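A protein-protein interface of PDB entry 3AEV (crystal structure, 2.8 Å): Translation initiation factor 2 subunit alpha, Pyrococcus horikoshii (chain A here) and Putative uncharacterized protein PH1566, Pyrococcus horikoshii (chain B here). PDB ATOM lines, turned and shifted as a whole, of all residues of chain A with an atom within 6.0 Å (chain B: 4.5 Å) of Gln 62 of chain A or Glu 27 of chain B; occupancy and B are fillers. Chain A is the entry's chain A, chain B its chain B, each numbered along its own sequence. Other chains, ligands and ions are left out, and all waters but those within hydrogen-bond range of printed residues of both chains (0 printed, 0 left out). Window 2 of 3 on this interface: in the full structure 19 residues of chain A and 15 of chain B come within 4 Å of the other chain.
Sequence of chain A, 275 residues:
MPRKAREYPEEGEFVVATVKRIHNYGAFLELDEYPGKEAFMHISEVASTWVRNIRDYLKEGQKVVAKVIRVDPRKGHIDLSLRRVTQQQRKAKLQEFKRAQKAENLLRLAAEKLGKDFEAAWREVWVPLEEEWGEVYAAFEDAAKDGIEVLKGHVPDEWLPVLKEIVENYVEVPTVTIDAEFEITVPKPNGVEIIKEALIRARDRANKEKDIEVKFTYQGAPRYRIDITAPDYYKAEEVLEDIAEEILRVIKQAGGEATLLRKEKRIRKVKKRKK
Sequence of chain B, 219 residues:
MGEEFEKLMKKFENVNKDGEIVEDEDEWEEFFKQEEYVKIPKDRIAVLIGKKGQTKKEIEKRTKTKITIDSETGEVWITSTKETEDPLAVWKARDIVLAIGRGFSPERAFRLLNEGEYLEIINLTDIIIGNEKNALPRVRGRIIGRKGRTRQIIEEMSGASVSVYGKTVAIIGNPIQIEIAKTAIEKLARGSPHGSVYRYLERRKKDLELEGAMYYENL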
ATOM      1  N   ALA A  17       4.051  23.534  10.171  1.00  0.00           N
ATOM      2  CA  ALA A  17       4.144  24.830  10.809  1.00  0.00           C
ATOM      3  C   ALA A  17       5.508  25.051  11.423  1.00  0.00           C
ATOM      4  O   ALA A  17       6.232  24.102  11.709  1.00  0.00           O
ATOM      5  CB  ALA A  17       3.069  24.971  11.872  1.00  0.00           C
ATOM      6  N   THR A  18       5.840  26.313  11.657  1.00  0.00           N
ATOM      7  CA  THR A  18       7.116  26.645  12.262  1.00  0.00           C
ATOM      8  C   THR A  18       6.928  27.352  13.594  1.00  0.00           C
ATOM      9  O   THR A  18       6.167  28.322  13.696  1.00  0.00           O
ATOM     10  CB  THR A  18       7.955  27.463  11.271  1.00  0.00           C
ATOM     11  OG1 THR A  18       8.117  26.681  10.068  1.00  0.00           O
ATOM     12  CG2 THR A  18       9.311  27.804  11.849  1.00  0.00           C
ATOM     13  N   VAL A  19       7.596  26.840  14.626  1.00  0.00           N
ATOM     14  CA  VAL A  19       7.532  27.443  15.950  1.00  0.00           C
ATOM     15  C   VAL A  19       8.194  28.814  15.934  1.00  0.00           C
ATOM     16  O   VAL A  19       9.394  28.927  15.677  1.00  0.00           O
ATOM     17  CB  VAL A  19       8.269  26.576  16.989  1.00  0.00           C
ATOM     18  CG1 VAL A  19       8.196  27.226  18.355  1.00  0.00           C
ATOM     19  CG2 VAL A  19       7.710  25.160  17.021  1.00  0.00           C
ATOM     20  N   LEU A  29       2.956  29.555  16.348  1.00  0.00           N
ATOM     21  CA  LEU A  29       3.599  28.971  15.175  1.00  0.00           C
ATOM     22  C   LEU A  29       3.123  29.695  13.936  1.00  0.00           C
ATOM     23  O   LEU A  29       1.973  30.132  13.890  1.00  0.00           O
ATOM     24  CB  LEU A  29       3.231  27.503  15.049  1.00  0.00           C
ATOM     25  CG  LEU A  29       3.746  26.581  16.154  1.00  0.00           C
ATOM     26  CD1 LEU A  29       2.814  26.618  17.377  1.00  0.00           C
ATOM     27  CD2 LEU A  29       3.910  25.172  15.639  1.00  0.00           C
ATOM     28  N   TYR A  57      10.189  20.230  24.227  1.00  0.00           N
ATOM     29  CA  TYR A  57       9.534  19.687  23.052  1.00  0.00           C
ATOM     30  C   TYR A  57       9.539  20.599  21.872  1.00  0.00           C
ATOM     31  O   TYR A  57       9.263  20.154  20.776  1.00  0.00           O
ATOM     32  CB  TYR A  57       8.081  19.419  23.361  1.00  0.00           C
ATOM     33  CG  TYR A  57       7.865  18.314  24.331  1.00  0.00           C
ATOM     34  CD1 TYR A  57       7.885  18.571  25.701  1.00  0.00           C
ATOM     35  CD2 TYR A  57       7.633  17.009  23.886  1.00  0.00           C
ATOM     36  CE1 TYR A  57       7.697  17.564  26.603  1.00  0.00           C
ATOM     37  CE2 TYR A  57       7.439  15.985  24.789  1.00  0.00           C
ATOM     38  CZ  TYR A  57       7.469  16.279  26.149  1.00  0.00           C
ATOM     39  OH  TYR A  57       7.263  15.298  27.074  1.00  0.00           O
ATOM     40  N   LEU A  58       9.796  21.884  22.097  1.00  0.00           N
ATOM     41  CA  LEU A  58       9.741  22.874  21.036  1.00  0.00           C
ATOM     42  C   LEU A  58      10.890  23.844  21.172  1.00  0.00           C
ATOM     43  O   LEU A  58      11.272  24.178  22.272  1.00  0.00           O
ATOM     44  CB  LEU A  58       8.424  23.636  21.101  1.00  0.00           C
ATOM     45  CG  LEU A  58       7.090  22.884  20.986  1.00  0.00           C
ATOM     46  CD1 LEU A  58       5.940  23.853  20.963  1.00  0.00           C
ATOM     47  CD2 LEU A  58       7.045  22.029  19.764  1.00  0.00           C
ATOM     48  N   LYS A  59      11.450  24.253  20.041  1.00  0.00           N
ATOM     49  CA  LYS A  59      12.540  25.218  19.940  1.00  0.00           C
ATOM     50  C   LYS A  59      12.073  26.247  18.957  1.00  0.00           C
ATOM     51  O   LYS A  59      11.425  25.900  17.958  1.00  0.00           O
ATOM     52  CB  LYS A  59      13.767  24.582  19.288  1.00  0.00           C
ATOM     53  CG  LYS A  59      14.744  23.911  20.223  1.00  0.00           C
ATOM     54  CD  LYS A  59      16.147  23.811  19.605  1.00  0.00           C
ATOM     55  CE  LYS A  59      16.318  22.557  18.720  1.00  0.00           C
ATOM     56  NZ  LYS A  59      17.764  22.095  18.706  1.00  0.00           N
ATOM     57  N   GLU A  60      12.415  27.511  19.172  1.00  0.00           N
ATOM     58  CA  GLU A  60      12.139  28.458  18.107  1.00  0.00           C
ATOM     59  C   GLU A  60      12.846  28.018  16.798  1.00  0.00           C
ATOM     60  O   GLU A  60      14.011  27.562  16.799  1.00  0.00           O
ATOM     61  CB  GLU A  60      12.381  29.925  18.500  1.00  0.00           C
ATOM     62  CG  GLU A  60      13.327  30.190  19.665  1.00  0.00           C
ATOM     63  CD  GLU A  60      12.684  30.030  21.064  1.00  0.00           C
ATOM     64  OE1 GLU A  60      11.741  30.796  21.421  1.00  0.00           O
ATOM     65  OE2 GLU A  60      13.162  29.149  21.819  1.00  0.00           O
ATOM     66  N   GLY A  61      12.075  28.085  15.710  1.00  0.00           N
ATOM     67  CA  GLY A  61      12.533  27.706  14.388  1.00  0.00           C
ATOM     68  C   GLY A  61      12.145  26.306  13.956  1.00  0.00           C
ATOM     69  O   GLY A  61      12.169  26.003  12.782  1.00  0.00           O
ATOM     70  N   GLN A  62      11.796  25.441  14.904  1.00  0.00           N
ATOM     71  CA  GLN A  62      11.473  24.037  14.623  1.00  0.00           C
ATOM     72  C   GLN A  62      10.257  23.892  13.723  1.00  0.00           C
ATOM     73  O   GLN A  62       9.269  24.621  13.878  1.00  0.00           O
ATOM     74  CB  GLN A  62      11.205  23.303  15.934  1.00  0.00           C
ATOM     75  CG  GLN A  62      10.957  21.840  15.797  1.00  0.00           C
ATOM     76  CD  GLN A  62      10.657  21.189  17.123  1.00  0.00           C
ATOM     77  OE1 GLN A  62      10.867  21.768  18.199  1.00  0.00           O
ATOM     78  NE2 GLN A  62      10.145  19.971  17.059  1.00  0.00           N
ATOM     79  N   LYS A  63      10.339  22.943  12.789  1.00  0.00           N
ATOM     80  CA  LYS A  63       9.247  22.636  11.860  1.00  0.00           C
ATOM     81  C   LYS A  63       8.506  21.384  12.344  1.00  0.00           C
ATOM     82  O   LYS A  63       9.111  20.448  12.856  1.00  0.00           O
ATOM     83  CB  LYS A  63       9.792  22.470  10.446  1.00  0.00           C
ATOM     84  CG  LYS A  63       9.139  23.352   9.418  1.00  0.00           C
ATOM     85  CD  LYS A  63       9.970  23.511   8.150  1.00  0.00           C
ATOM     86  CE  LYS A  63      10.768  24.814   8.164  1.00  0.00           C
ATOM     87  NZ  LYS A  63       9.920  26.007   7.832  1.00  0.00           N
ATOM     88  N   VAL A  64       7.196  21.363  12.172  1.00  0.00           N
ATOM     89  CA  VAL A  64       6.342  20.427  12.870  1.00  0.00           C
ATOM     90  C   VAL A  64       5.125  20.134  11.993  1.00  0.00           C
ATOM     91  O   VAL A  64       4.662  21.019  11.222  1.00  0.00           O
ATOM     92  CB  VAL A  64       5.928  21.104  14.183  1.00  0.00           C
ATOM     93  CG1 VAL A  64       4.438  21.307  14.301  1.00  0.00           C
ATOM     94  CG2 VAL A  64       6.524  20.428  15.371  1.00  0.00           C
ATOM     95  N   LEU A  82      -0.147  19.026  18.466  1.00  0.00           N
ATOM     96  CA  LEU A  82       0.902  18.156  18.043  1.00  0.00           C
ATOM     97  C   LEU A  82       0.601  16.735  18.544  1.00  0.00           C
ATOM     98  O   LEU A  82       0.828  15.741  17.820  1.00  0.00           O
ATOM     99  CB  LEU A  82       2.228  18.708  18.547  1.00  0.00           C
ATOM    100  CG  LEU A  82       3.510  17.996  18.133  1.00  0.00           C
ATOM    101  CD1 LEU A  82       3.716  18.170  16.657  1.00  0.00           C
ATOM    102  CD2 LEU A  82       4.753  18.503  18.932  1.00  0.00           C
ATOM    103  N   ASP B  26      18.331  16.639   9.659  1.00  0.00           N
ATOM    104  CA  ASP B  26      17.163  15.744   9.907  1.00  0.00           C
ATOM    105  C   ASP B  26      15.829  16.468   9.749  1.00  0.00           C
ATOM    106  O   ASP B  26      14.866  15.859   9.302  1.00  0.00           O
ATOM    107  CB  ASP B  26      17.242  15.039  11.269  1.00  0.00           C
ATOM    108  CG  ASP B  26      16.353  13.790  11.337  1.00  0.00           C
ATOM    109  OD1 ASP B  26      16.084  13.298  12.443  1.00  0.00           O
ATOM    110  OD2 ASP B  26      15.915  13.292  10.281  1.00  0.00           O
ATOM    111  N   GLU B  27      15.761  17.749  10.116  1.00  0.00           N
ATOM    112  CA  GLU B  27      14.609  18.584   9.745  1.00  0.00           C
ATOM    113  C   GLU B  27      14.503  18.575   8.232  1.00  0.00           C
ATOM    114  O   GLU B  27      13.450  18.294   7.674  1.00  0.00           O
ATOM    115  CB  GLU B  27      14.778  20.028  10.215  1.00  0.00           C
ATOM    116  CG  GLU B  27      13.495  20.839  10.264  1.00  0.00           C
ATOM    117  CD  GLU B  27      12.950  20.996  11.686  1.00  0.00           C
ATOM    118  OE1 GLU B  27      12.809  22.154  12.141  1.00  0.00           O
ATOM    119  OE2 GLU B  27      12.669  19.971  12.360  1.00  0.00           O
ATOM    120  N   TRP B  28      15.616  18.870   7.580  1.00  0.00           N
ATOM    121  CA  TRP B  28      15.686  18.901   6.132  1.00  0.00           C
ATOM    122  C   TRP B  28      15.374  17.536   5.499  1.00  0.00           C
ATOM    123  O   TRP B  28      14.543  17.437   4.610  1.00  0.00           O
ATOM    124  CB  TRP B  28      17.045  19.444   5.683  1.00  0.00           C
ATOM    125  CG  TRP B  28      17.242  19.406   4.195  1.00  0.00           C
ATOM    126  CD1 TRP B  28      16.812  20.330   3.272  1.00  0.00           C
ATOM    127  CD2 TRP B  28      17.910  18.381   3.454  1.00  0.00           C
ATOM    128  NE1 TRP B  28      17.177  19.936   2.007  1.00  0.00           N
ATOM    129  CE2 TRP B  28      17.851  18.744   2.091  1.00  0.00           C
ATOM    130  CE3 TRP B  28      18.554  17.183   3.812  1.00  0.00           C
ATOM    131  CZ2 TRP B  28      18.415  17.955   1.088  1.00  0.00           C
ATOM    132  CZ3 TRP B  28      19.127  16.401   2.807  1.00  0.00           C
ATOM    133  CH2 TRP B  28      19.050  16.792   1.465  1.00  0.00           C
ATOM    134  N   GLU B  29      16.031  16.491   5.976  1.00  0.00           N
ATOM    135  CA  GLU B  29      15.707  15.121   5.586  1.00  0.00           C
ATOM    136  C   GLU B  29      14.192  14.889   5.553  1.00  0.00           C
ATOM    137  O   GLU B  29      13.642  14.455   4.565  1.00  0.00           O
ATOM    138  CB  GLU B  29      16.389  14.121   6.553  1.00  0.00           C
ATOM    139  CG  GLU B  29      16.962  12.837   5.899  1.00  0.00           C
ATOM    140  CD  GLU B  29      18.001  12.083   6.766  1.00  0.00           C
ATOM    141  OE1 GLU B  29      18.474  12.601   7.814  1.00  0.00           O
ATOM    142  OE2 GLU B  29      18.363  10.945   6.384  1.00  0.00           O
ATOM    143  N   GLU B  30      13.520  15.219   6.641  1.00  0.00           N
ATOM    144  CA  GLU B  30      12.104  14.923   6.823  1.00  0.00           C
ATOM    145  C   GLU B  30      11.137  15.811   6.031  1.00  0.00           C
ATOM    146  O   GLU B  30      10.052  15.350   5.681  1.00  0.00           O
ATOM    147  CB  GLU B  30      11.750  14.983   8.313  1.00  0.00           C
ATOM    148  CG  GLU B  30      11.958  13.677   9.084  1.00  0.00           C
ATOM    149  CD  GLU B  30      11.377  13.751  10.509  1.00  0.00           C
ATOM    150  OE1 GLU B  30      11.187  12.681  11.142  1.00  0.00           O
ATOM    151  OE2 GLU B  30      11.104  14.876  11.009  1.00  0.00           O
ATOM    152  N   PHE B  31      11.501  17.065   5.757  1.00  0.00           N
ATOM    153  CA  PHE B  31      10.558  17.983   5.113  1.00  0.00           C
ATOM    154  C   PHE B  31      10.932  18.357   3.678  1.00  0.00           C
ATOM    155  O   PHE B  31      10.092  18.839   2.918  1.00  0.00           O
ATOM    156  CB  PHE B  31      10.390  19.269   5.931  1.00  0.00           C
ATOM    157  CG  PHE B  31       9.678  19.082   7.229  1.00  0.00           C
ATOM    158  CD1 PHE B  31       8.339  19.402   7.348  1.00  0.00           C
ATOM    159  CD2 PHE B  31      10.350  18.605   8.346  1.00  0.00           C
ATOM    160  CE1 PHE B  31       7.671  19.244   8.541  1.00  0.00           C
ATOM    161  CE2 PHE B  31       9.690  18.442   9.554  1.00  0.00           C
ATOM    162  CZ  PHE B  31       8.345  18.768   9.653  1.00  0.00           C
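Among the printed residues, merely in contact across the chains: Gly 61 of chain A with Glu 27 of chain B (3.95 Å), Gln 62 of chain A with Glu 27 of chain B (3.4 Å), Lys 63 of chain A with Phe 31 of chain B (3.7 Å) and Val 64 of chain A with Phe 31 of chain B (3.8 Å).
Ala 17 of chain A touches none of the printed residues of chain B. Val 19 of chain A touches none of the printed residues of chain B. Of the printed residues of chain B, Gly 61 of chain A touches Glu 27. Gln 62 of chain A touches one residue of chain B. Of the printed residues of chain B, Lys 63 of chain A touches Glu 27 (2.7 Å) and Phe 31 (3.7 Å). Printed residues of chain B within 4 Å of Val 64 of chain A: Phe 31 (3.8 Å). Of chain A, only Gly 61 (3.95 Å), Gln 62 (3.4 Å) and Lys 63 (2.7 Å) come within 4 Å of Glu 27 of chain B. Of the printed residues of chain A, Phe 31 of chain B touches Lys 63 and Val 64.
N of Ala 17 of chain A is in hydrogen-bond range of O of Val 64 of chain A, at 2.8 Å. The side-chain hydroxyl of Thr 18 of chain A is in hydrogen-bond range of the side-chain amino group of Lys 63 of chain A (3.0 Å). N of Gly 61 of chain A lies within hydrogen-bond range of O of Val 19 of chain A (2.8 Å). N of Val 19 of chain A sits at hydrogen-bond distance from O of Gln 62 of chain A, at 2.9 Å. The backbone carbonyl oxygen (O) of Tyr 57 of chain A lies close to the side-chain amide oxygen (OE1) of Gln 62 of chain A (3.4 Å). The backbone NH of Lys 59 of chain A is in hydrogen-bond range of the side-chain amide oxygen of Gln 62 of chain A (3.1 Å).
OE1 of Glu 27 of chain B sits at hydrogen-bond distance from N of Lys 63 of chain A.
Of the 13 printed residues of chain A, 4 touch a printed residue of chain B. Printed residues of chain A that touch a printed residue of chain B: Gly 61, Gln 62, Lys 63 and Val 64. Among the printed residues, 5 pairs touch across the chains. Among the printed residues, no Asp or Glu carboxylate lies within 4 Å of a Lys or Arg side-chain nitrogen of the other chain.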
